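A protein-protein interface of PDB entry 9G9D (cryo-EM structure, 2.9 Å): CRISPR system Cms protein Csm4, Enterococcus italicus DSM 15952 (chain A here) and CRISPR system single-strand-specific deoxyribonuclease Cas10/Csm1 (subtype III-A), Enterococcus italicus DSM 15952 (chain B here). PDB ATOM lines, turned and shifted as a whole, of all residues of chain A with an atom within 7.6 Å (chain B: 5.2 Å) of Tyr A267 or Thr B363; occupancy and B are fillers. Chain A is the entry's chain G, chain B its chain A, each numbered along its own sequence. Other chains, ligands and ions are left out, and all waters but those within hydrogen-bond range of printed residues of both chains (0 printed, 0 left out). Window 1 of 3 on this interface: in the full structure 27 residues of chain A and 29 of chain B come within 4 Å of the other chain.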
ATOM      1  N   ALA A 226      31.905  10.633 -12.553  1.00  0.00           N
ATOM      2  CA  ALA A 226      30.910  10.592 -11.494  1.00  0.00           C
ATOM      3  C   ALA A 226      30.174  11.919 -11.434  1.00  0.00           C
ATOM      4  O   ALA A 226      30.604  12.913 -12.025  1.00  0.00           O
ATOM      5  CB  ALA A 226      31.550  10.287 -10.135  1.00  0.00           C
ATOM      6  N   MET A 227      29.055  11.920 -10.714  1.00  0.00           N
ATOM      7  CA  MET A 227      28.290  13.127 -10.436  1.00  0.00           C
ATOM      8  C   MET A 227      27.471  12.893  -9.177  1.00  0.00           C
ATOM      9  O   MET A 227      26.912  11.808  -8.990  1.00  0.00           O
ATOM     10  CB  MET A 227      27.381  13.498 -11.611  1.00  0.00           C
ATOM     11  CG  MET A 227      27.423  14.974 -11.972  1.00  0.00           C
ATOM     12  SD  MET A 227      26.552  16.026 -10.800  1.00  0.00           S
ATOM     13  CE  MET A 227      24.854  15.636 -11.211  1.00  0.00           C
ATOM     14  N   ALA A 228      27.412  13.903  -8.316  1.00  0.00           N
ATOM     15  CA  ALA A 228      26.728  13.761  -7.039  1.00  0.00           C
ATOM     16  C   ALA A 228      25.259  14.137  -7.160  1.00  0.00           C
ATOM     17  O   ALA A 228      24.839  14.810  -8.105  1.00  0.00           O
ATOM     18  CB  ALA A 228      27.392  14.632  -5.975  1.00  0.00           C
ATOM     19  N   LEU A 243      35.899  18.937 -14.956  1.00  0.00           N
ATOM     20  CA  LEU A 243      35.472  18.871 -16.346  1.00  0.00           C
ATOM     21  C   LEU A 243      34.146  18.129 -16.410  1.00  0.00           C
ATOM     22  O   LEU A 243      34.063  16.964 -16.010  1.00  0.00           O
ATOM     23  CB  LEU A 243      36.520  18.170 -17.213  1.00  0.00           C
ATOM     24  CG  LEU A 243      36.242  18.151 -18.716  1.00  0.00           C
ATOM     25  CD1 LEU A 243      36.235  19.562 -19.278  1.00  0.00           C
ATOM     26  CD2 LEU A 243      37.263  17.288 -19.440  1.00  0.00           C
ATOM     27  N   LEU A 244      33.116  18.803 -16.906  1.00  0.00           N
ATOM     28  CA  LEU A 244      31.782  18.229 -17.007  1.00  0.00           C
ATOM     29  C   LEU A 244      31.624  17.619 -18.394  1.00  0.00           C
ATOM     30  O   LEU A 244      31.548  18.347 -19.390  1.00  0.00           O
ATOM     31  CB  LEU A 244      30.712  19.289 -16.753  1.00  0.00           C
ATOM     32  CG  LEU A 244      29.288  18.797 -16.505  1.00  0.00           C
ATOM     33  CD1 LEU A 244      29.209  18.018 -15.204  1.00  0.00           C
ATOM     34  CD2 LEU A 244      28.331  19.971 -16.483  1.00  0.00           C
ATOM     35  N   LYS A 245      31.580  16.293 -18.455  1.00  0.00           N
ATOM     36  CA  LYS A 245      31.525  15.562 -19.710  1.00  0.00           C
ATOM     37  C   LYS A 245      30.132  14.977 -19.893  1.00  0.00           C
ATOM     38  O   LYS A 245      29.498  14.546 -18.919  1.00  0.00           O
ATOM     39  CB  LYS A 245      32.582  14.455 -19.752  1.00  0.00           C
ATOM     40  CG  LYS A 245      32.444  13.404 -18.664  1.00  0.00           C
ATOM     41  CD  LYS A 245      33.531  12.350 -18.778  1.00  0.00           C
ATOM     42  CE  LYS A 245      33.494  11.666 -20.132  1.00  0.00           C
ATOM     43  NZ  LYS A 245      34.565  10.642 -20.264  1.00  0.00           N
ATOM     44  N   LYS A 246      29.659  14.977 -21.135  1.00  0.00           N
ATOM     45  CA  LYS A 246      28.345  14.432 -21.435  1.00  0.00           C
ATOM     46  C   LYS A 246      28.434  12.941 -21.732  1.00  0.00           C
ATOM     47  O   LYS A 246      29.286  12.487 -22.499  1.00  0.00           O
ATOM     48  CB  LYS A 246      27.714  15.169 -22.618  1.00  0.00           C
ATOM     49  CG  LYS A 246      28.543  15.166 -23.891  1.00  0.00           C
ATOM     50  CD  LYS A 246      27.771  15.777 -25.046  1.00  0.00           C
ATOM     51  CE  LYS A 246      28.548  15.660 -26.344  1.00  0.00           C
ATOM     52  NZ  LYS A 246      27.767  16.161 -27.506  1.00  0.00           N
ATOM     53  N   ARG A 247      27.547  12.180 -21.105  1.00  0.00           N
ATOM     54  CA  ARG A 247      27.415  10.750 -21.324  1.00  0.00           C
ATOM     55  C   ARG A 247      26.082  10.507 -22.018  1.00  0.00           C
ATOM     56  O   ARG A 247      25.021  10.600 -21.386  1.00  0.00           O
ATOM     57  CB  ARG A 247      27.490   9.982 -20.006  1.00  0.00           C
ATOM     58  CG  ARG A 247      28.478  10.548 -19.000  1.00  0.00           C
ATOM     59  CD  ARG A 247      29.913  10.474 -19.495  1.00  0.00           C
ATOM     60  NE  ARG A 247      30.345   9.102 -19.726  1.00  0.00           N
ATOM     61  CZ  ARG A 247      30.612   8.589 -20.920  1.00  0.00           C
ATOM     62  NH1 ARG A 247      30.527   9.319 -22.020  1.00  0.00           N
ATOM     63  NH2 ARG A 247      30.978   7.315 -21.011  1.00  0.00           N
ATOM     64  N   THR A 248      26.139  10.235 -23.318  1.00  0.00           N
ATOM     65  CA  THR A 248      24.969   9.952 -24.135  1.00  0.00           C
ATOM     66  C   THR A 248      25.206   8.645 -24.873  1.00  0.00           C
ATOM     67  O   THR A 248      26.358   8.258 -25.092  1.00  0.00           O
ATOM     68  CB  THR A 248      24.702  11.080 -25.136  1.00  0.00           C
ATOM     69  OG1 THR A 248      25.763  11.124 -26.099  1.00  0.00           O
ATOM     70  CG2 THR A 248      24.630  12.417 -24.422  1.00  0.00           C
ATOM     71  N   LYS A 264      18.750   8.811 -21.948  1.00  0.00           N
ATOM     72  CA  LYS A 264      18.672  10.197 -21.512  1.00  0.00           C
ATOM     73  C   LYS A 264      20.075  10.763 -21.339  1.00  0.00           C
ATOM     74  O   LYS A 264      20.957  10.113 -20.772  1.00  0.00           O
ATOM     75  CB  LYS A 264      17.895  10.301 -20.200  1.00  0.00           C
ATOM     76  CG  LYS A 264      16.410  10.033 -20.335  1.00  0.00           C
ATOM     77  CD  LYS A 264      15.728  10.033 -18.979  1.00  0.00           C
ATOM     78  CE  LYS A 264      16.058  11.292 -18.200  1.00  0.00           C
ATOM     79  NZ  LYS A 264      15.379  11.317 -16.878  1.00  0.00           N
ATOM     80  N   ASP A 265      20.282  11.977 -21.842  1.00  0.00           N
ATOM     81  CA  ASP A 265      21.593  12.602 -21.746  1.00  0.00           C
ATOM     82  C   ASP A 265      21.974  12.810 -20.287  1.00  0.00           C
ATOM     83  O   ASP A 265      21.176  13.295 -19.481  1.00  0.00           O
ATOM     84  CB  ASP A 265      21.606  13.939 -22.486  1.00  0.00           C
ATOM     85  CG  ASP A 265      21.462  13.776 -23.985  1.00  0.00           C
ATOM     86  OD1 ASP A 265      21.230  12.637 -24.440  1.00  0.00           O
ATOM     87  OD2 ASP A 265      21.585  14.785 -24.709  1.00  0.00           O
ATOM     88  N   PHE A 266      23.204  12.438 -19.949  1.00  0.00           N
ATOM     89  CA  PHE A 266      23.716  12.605 -18.598  1.00  0.00           C
ATOM     90  C   PHE A 266      24.933  13.511 -18.648  1.00  0.00           C
ATOM     91  O   PHE A 266      25.570  13.641 -19.694  1.00  0.00           O
ATOM     92  CB  PHE A 266      24.077  11.255 -17.974  1.00  0.00           C
ATOM     93  CG  PHE A 266      24.363  11.319 -16.505  1.00  0.00           C
ATOM     94  CD1 PHE A 266      23.333  11.456 -15.593  1.00  0.00           C
ATOM     95  CD2 PHE A 266      25.660  11.223 -16.037  1.00  0.00           C
ATOM     96  CE1 PHE A 266      23.594  11.508 -14.241  1.00  0.00           C
ATOM     97  CE2 PHE A 266      25.926  11.272 -14.686  1.00  0.00           C
ATOM     98  CZ  PHE A 266      24.893  11.415 -13.787  1.00  0.00           C
ATOM     99  N   TYR A 267      25.248  14.148 -17.526  1.00  0.00           N
ATOM    100  CA  TYR A 267      26.439  14.975 -17.406  1.00  0.00           C
ATOM    101  C   TYR A 267      27.139  14.639 -16.100  1.00  0.00           C
ATOM    102  O   TYR A 267      26.522  14.691 -15.031  1.00  0.00           O
ATOM    103  CB  TYR A 267      26.087  16.462 -17.468  1.00  0.00           C
ATOM    104  CG  TYR A 267      25.754  16.936 -18.861  1.00  0.00           C
ATOM    105  CD1 TYR A 267      24.475  16.792 -19.378  1.00  0.00           C
ATOM    106  CD2 TYR A 267      26.722  17.520 -19.664  1.00  0.00           C
ATOM    107  CE1 TYR A 267      24.168  17.222 -20.653  1.00  0.00           C
ATOM    108  CE2 TYR A 267      26.424  17.952 -20.937  1.00  0.00           C
ATOM    109  CZ  TYR A 267      25.147  17.800 -21.427  1.00  0.00           C
ATOM    110  OH  TYR A 267      24.849  18.231 -22.699  1.00  0.00           O
ATOM    111  N   ALA A 268      28.419  14.287 -16.185  1.00  0.00           N
ATOM    112  CA  ALA A 268      29.159  13.819 -15.023  1.00  0.00           C
ATOM    113  C   ALA A 268      30.520  14.491 -14.957  1.00  0.00           C
ATOM    114  O   ALA A 268      31.077  14.906 -15.976  1.00  0.00           O
ATOM    115  CB  ALA A 268      29.338  12.299 -15.048  1.00  0.00           C
ATOM    116  N   PHE A 269      31.055  14.590 -13.745  1.00  0.00           N
ATOM    117  CA  PHE A 269      32.393  15.133 -13.578  1.00  0.00           C
ATOM    118  C   PHE A 269      33.424  14.126 -14.066  1.00  0.00           C
ATOM    119  O   PHE A 269      33.396  12.953 -13.688  1.00  0.00           O
ATOM    120  CB  PHE A 269      32.645  15.492 -12.115  1.00  0.00           C
ATOM    121  CG  PHE A 269      31.681  16.503 -11.568  1.00  0.00           C
ATOM    122  CD1 PHE A 269      31.680  17.802 -12.043  1.00  0.00           C
ATOM    123  CD2 PHE A 269      30.782  16.157 -10.576  1.00  0.00           C
ATOM    124  CE1 PHE A 269      30.798  18.733 -11.544  1.00  0.00           C
ATOM    125  CE2 PHE A 269      29.897  17.086 -10.073  1.00  0.00           C
ATOM    126  CZ  PHE A 269      29.906  18.376 -10.558  1.00  0.00           C
ATOM    127  N   SER A 270      34.330  14.592 -14.921  1.00  0.00           N
ATOM    128  CA  SER A 270      35.326  13.711 -15.509  1.00  0.00           C
ATOM    129  C   SER A 270      36.290  13.201 -14.445  1.00  0.00           C
ATOM    130  O   SER A 270      36.517  13.847 -13.420  1.00  0.00           O
ATOM    131  CB  SER A 270      36.097  14.440 -16.610  1.00  0.00           C
ATOM    132  OG  SER A 270      37.092  13.603 -17.170  1.00  0.00           O
ATOM    133  N   PHE A 284      22.559   6.266 -11.476  1.00  0.00           N
ATOM    134  CA  PHE A 284      21.501   7.070 -12.068  1.00  0.00           C
ATOM    135  C   PHE A 284      20.717   6.245 -13.076  1.00  0.00           C
ATOM    136  O   PHE A 284      21.224   5.257 -13.613  1.00  0.00           O
ATOM    137  CB  PHE A 284      22.071   8.325 -12.734  1.00  0.00           C
ATOM    138  CG  PHE A 284      22.405   9.422 -11.765  1.00  0.00           C
ATOM    139  CD1 PHE A 284      21.455  10.368 -11.420  1.00  0.00           C
ATOM    140  CD2 PHE A 284      23.662   9.508 -11.198  1.00  0.00           C
ATOM    141  CE1 PHE A 284      21.756  11.377 -10.532  1.00  0.00           C
ATOM    142  CE2 PHE A 284      23.968  10.517 -10.309  1.00  0.00           C
ATOM    143  CZ  PHE A 284      23.014  11.452  -9.976  1.00  0.00           C
ATOM    144  N   VAL A 286      18.914   6.580 -16.622  1.00  0.00           N
ATOM    145  CA  VAL A 286      18.714   7.363 -17.835  1.00  0.00           C
ATOM    146  C   VAL A 286      17.681   6.740 -18.761  1.00  0.00           C
ATOM    147  O   VAL A 286      17.690   7.024 -19.966  1.00  0.00           O
ATOM    148  CB  VAL A 286      20.046   7.572 -18.583  1.00  0.00           C
ATOM    149  CG1 VAL A 286      20.990   8.415 -17.749  1.00  0.00           C
ATOM    150  CG2 VAL A 286      20.681   6.237 -18.910  1.00  0.00           C
ATOM    151  N   ARG A 296      23.161   3.952 -15.285  1.00  0.00           N
ATOM    152  CA  ARG A 296      24.414   4.635 -15.562  1.00  0.00           C
ATOM    153  C   ARG A 296      25.190   4.764 -14.261  1.00  0.00           C
ATOM    154  O   ARG A 296      24.623   5.129 -13.224  1.00  0.00           O
ATOM    155  CB  ARG A 296      24.172   6.006 -16.195  1.00  0.00           C
ATOM    156  CG  ARG A 296      25.440   6.722 -16.630  1.00  0.00           C
ATOM    157  CD  ARG A 296      25.173   7.620 -17.823  1.00  0.00           C
ATOM    158  NE  ARG A 296      25.637   7.019 -19.068  1.00  0.00           N
ATOM    159  CZ  ARG A 296      25.296   7.445 -20.276  1.00  0.00           C
ATOM    160  NH1 ARG A 296      24.460   8.456 -20.442  1.00  0.00           N
ATOM    161  NH2 ARG A 296      25.807   6.841 -21.344  1.00  0.00           N
ATOM    162  N   ALA A 298      27.629   6.451 -11.808  1.00  0.00           N
ATOM    163  CA  ALA A 298      28.195   7.739 -11.440  1.00  0.00           C
ATOM    164  C   ALA A 298      28.768   7.735 -10.031  1.00  0.00           C
ATOM    165  O   ALA A 298      28.859   8.796  -9.407  1.00  0.00           O
ATOM    166  CB  ALA A 298      27.146   8.842 -11.582  1.00  0.00           C
ATOM    167  N   PHE B 361      23.461  25.613 -27.030  1.00  0.00           N
ATOM    168  CA  PHE B 361      24.455  24.548 -27.102  1.00  0.00           C
ATOM    169  C   PHE B 361      24.702  23.996 -25.707  1.00  0.00           C
ATOM    170  O   PHE B 361      25.418  24.611 -24.912  1.00  0.00           O
ATOM    171  CB  PHE B 361      25.774  25.052 -27.698  1.00  0.00           C
ATOM    172  CG  PHE B 361      25.612  25.866 -28.948  1.00  0.00           C
ATOM    173  CD1 PHE B 361      25.457  25.251 -30.177  1.00  0.00           C
ATOM    174  CD2 PHE B 361      25.635  27.250 -28.895  1.00  0.00           C
ATOM    175  CE1 PHE B 361      25.316  26.001 -31.332  1.00  0.00           C
ATOM    176  CE2 PHE B 361      25.496  28.006 -30.045  1.00  0.00           C
ATOM    177  CZ  PHE B 361      25.336  27.379 -31.265  1.00  0.00           C
ATOM    178  N   LYS B 362      24.141  22.821 -25.422  1.00  0.00           N
ATOM    179  CA  LYS B 362      24.262  22.221 -24.094  1.00  0.00           C
ATOM    180  C   LYS B 362      25.686  21.701 -23.928  1.00  0.00           C
ATOM    181  O   LYS B 362      26.017  20.559 -24.260  1.00  0.00           O
ATOM    182  CB  LYS B 362      23.221  21.126 -23.899  1.00  0.00           C
ATOM    183  CG  LYS B 362      21.810  21.651 -23.696  1.00  0.00           C
ATOM    184  CD  LYS B 362      20.957  20.656 -22.927  1.00  0.00           C
ATOM    185  CE  LYS B 362      19.628  21.268 -22.518  1.00  0.00           C
ATOM    186  NZ  LYS B 362      18.839  20.342 -21.661  1.00  0.00           N
ATOM    187  N   THR B 363      26.545  22.579 -23.412  1.00  0.00           N
ATOM    188  CA  THR B 363      27.967  22.384 -23.121  1.00  0.00           C
ATOM    189  C   THR B 363      28.808  22.234 -24.385  1.00  0.00           C
ATOM    190  O   THR B 363      30.009  21.967 -24.271  1.00  0.00           O
ATOM    191  CB  THR B 363      28.244  21.180 -22.206  1.00  0.00           C
ATOM    192  OG1 THR B 363      27.856  19.969 -22.867  1.00  0.00           O
ATOM    193  CG2 THR B 363      27.472  21.316 -20.904  1.00  0.00           C
ATOM    194  N   ASP B 364      28.233  22.388 -25.579  1.00  0.00           N
ATOM    195  CA  ASP B 364      29.042  22.316 -26.791  1.00  0.00           C
ATOM    196  C   ASP B 364      29.878  23.578 -26.972  1.00  0.00           C
ATOM    197  O   ASP B 364      30.953  23.537 -27.582  1.00  0.00           O
ATOM    198  CB  ASP B 364      28.149  22.083 -28.011  1.00  0.00           C
ATOM    199  CG  ASP B 364      27.493  20.716 -27.998  1.00  0.00           C
ATOM    200  OD1 ASP B 364      28.050  19.793 -27.369  1.00  0.00           O
ATOM    201  OD2 ASP B 364      26.422  20.564 -28.622  1.00  0.00           O
ATOM    202  N   LEU B 365      29.402  24.706 -26.452  1.00  0.00           N
ATOM    203  CA  LEU B 365      30.124  25.969 -26.514  1.00  0.00           C
ATOM    204  C   LEU B 365      29.954  26.717 -25.201  1.00  0.00           C
ATOM    205  O   LEU B 365      28.936  26.569 -24.519  1.00  0.00           O
ATOM    206  CB  LEU B 365      29.633  26.836 -27.680  1.00  0.00           C
ATOM    207  CG  LEU B 365      29.978  26.362 -29.092  1.00  0.00           C
ATOM    208  CD1 LEU B 365      29.288  27.235 -30.121  1.00  0.00           C
ATOM    209  CD2 LEU B 365      31.479  26.378 -29.309  1.00  0.00           C
ATOM    210  N   SER B 366      30.955  27.524 -24.852  1.00  0.00           N
ATOM    211  CA  SER B 366      30.929  28.302 -23.621  1.00  0.00           C
ATOM    212  C   SER B 366      31.798  29.540 -23.780  1.00  0.00           C
ATOM    213  O   SER B 366      32.686  29.590 -24.634  1.00  0.00           O
ATOM    214  CB  SER B 366      31.412  27.477 -22.422  1.00  0.00           C
ATOM    215  OG  SER B 366      30.573  26.356 -22.207  1.00  0.00           O
ATOM    216  N   TYR B 405      30.644  26.391 -14.861  1.00  0.00           N
ATOM    217  CA  TYR B 405      29.221  26.121 -14.687  1.00  0.00           C
ATOM    218  C   TYR B 405      28.880  26.216 -13.208  1.00  0.00           C
ATOM    219  O   TYR B 405      29.746  26.087 -12.340  1.00  0.00           O
ATOM    220  CB  TYR B 405      28.828  24.753 -15.258  1.00  0.00           C
ATOM    221  CG  TYR B 405      28.817  24.719 -16.768  1.00  0.00           C
ATOM    222  CD1 TYR B 405      27.849  25.406 -17.487  1.00  0.00           C
ATOM    223  CD2 TYR B 405      29.781  24.017 -17.474  1.00  0.00           C
ATOM    224  CE1 TYR B 405      27.839  25.391 -18.866  1.00  0.00           C
ATOM    225  CE2 TYR B 405      29.779  23.994 -18.855  1.00  0.00           C
ATOM    226  CZ  TYR B 405      28.806  24.683 -19.546  1.00  0.00           C
ATOM    227  OH  TYR B 405      28.798  24.664 -20.921  1.00  0.00           O
ATOM    228  N   PHE B 413      21.053  20.394 -16.501  1.00  0.00           N
ATOM    229  CA  PHE B 413      21.474  19.446 -17.529  1.00  0.00           C
ATOM    230  C   PHE B 413      20.889  18.059 -17.290  1.00  0.00           C
ATOM    231  O   PHE B 413      20.483  17.378 -18.238  1.00  0.00           O
ATOM    232  CB  PHE B 413      22.999  19.382 -17.577  1.00  0.00           C
ATOM    233  CG  PHE B 413      23.638  20.619 -18.136  1.00  0.00           C
ATOM    234  CD1 PHE B 413      23.128  21.224 -19.272  1.00  0.00           C
ATOM    235  CD2 PHE B 413      24.746  21.180 -17.523  1.00  0.00           C
ATOM    236  CE1 PHE B 413      23.714  22.360 -19.790  1.00  0.00           C
ATOM    237  CE2 PHE B 413      25.335  22.317 -18.037  1.00  0.00           C
ATOM    238  CZ  PHE B 413      24.818  22.908 -19.171  1.00  0.00           C
ATOM    239  N   ASN B 414      20.842  17.621 -16.032  1.00  0.00           N
ATOM    240  CA  ASN B 414      20.381  16.266 -15.747  1.00  0.00           C
ATOM    241  C   ASN B 414      18.886  16.236 -15.453  1.00  0.00           C
ATOM    242  O   ASN B 414      18.336  15.186 -15.099  1.00  0.00           O
ATOM    243  CB  ASN B 414      21.175  15.684 -14.579  1.00  0.00           C
ATOM    244  CG  ASN B 414      22.672  15.790 -14.786  1.00  0.00           C
ATOM    245  OD1 ASN B 414      23.270  14.985 -15.497  1.00  0.00           O
ATOM    246  ND2 ASN B 414      23.287  16.790 -14.164  1.00  0.00           N
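NZ of Lys A246 is in salt-bridge range of OD1 of Asp B364. OH of Tyr A267 lies within hydrogen-bond range of O of Lys B362 (3.0 Å). The side-chain hydroxyl (OH) of Tyr A267 lies close to the side-chain hydroxyl (OG1) of Thr B363. N of Tyr A267 lies within hydrogen-bond range of OD1 of Asn B414 (3.0 Å).
The backbone NH of Met A227 sits at hydrogen-bond distance from the backbone carbonyl oxygen of Ala A298 (3.4 Å). The backbone NH (N) of Arg A247 lies within hydrogen-bond range of the backbone carbonyl oxygen (O) of Phe A266, 2.8 Å away.
Met A227 touches Asn B414 (CE to ND2, 3.5 Å). Phe B413 touches Leu A244 (CD2 to CD2, 3.9 Å). Phe A266 touches Asn B414 (CD1 to OD1, 3.5 Å). CB of Phe B413 touches CD1 of Tyr A267 (3.5 Å).
Of chain B, only Lys B362, Thr B363, Phe B413 and Asn B414 come within 4 Å of Tyr A267. Thr B363 touches just one residue of chain A: Tyr A267. Of the printed residues of chain A, Phe B413 touches Leu A244 (3.9 Å) and Tyr A267 (3.5 Å). Of the printed residues of chain B, Met A227 touches Asn B414 (3.5 Å). Printed residues of chain B within 4 Å of Leu A244: Phe B413 (3.9 Å). Printed residues of chain B within 4 Å of Phe A266: Asn B414. Thr A248 touches none of the printed residues of chain B. Ala A298 touches none of the printed residues of chain B. The nearest printed residue of chain B that does not touch Met A227 is Phe B413 (7.6 Å).
Hydrophobic or aromatic side chains of chain A within 4 Å of the printed part of chain B: Met A227, Leu A244, Phe A266 and Tyr A267. Among the printed residues, 8 pairs touch across the chains. Among the printed residues, Asp or Glu carboxylates within 4 Å of a Lys or Arg side-chain nitrogen of the other chain: Lys A246 with Asp B364 (3.6 Å).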
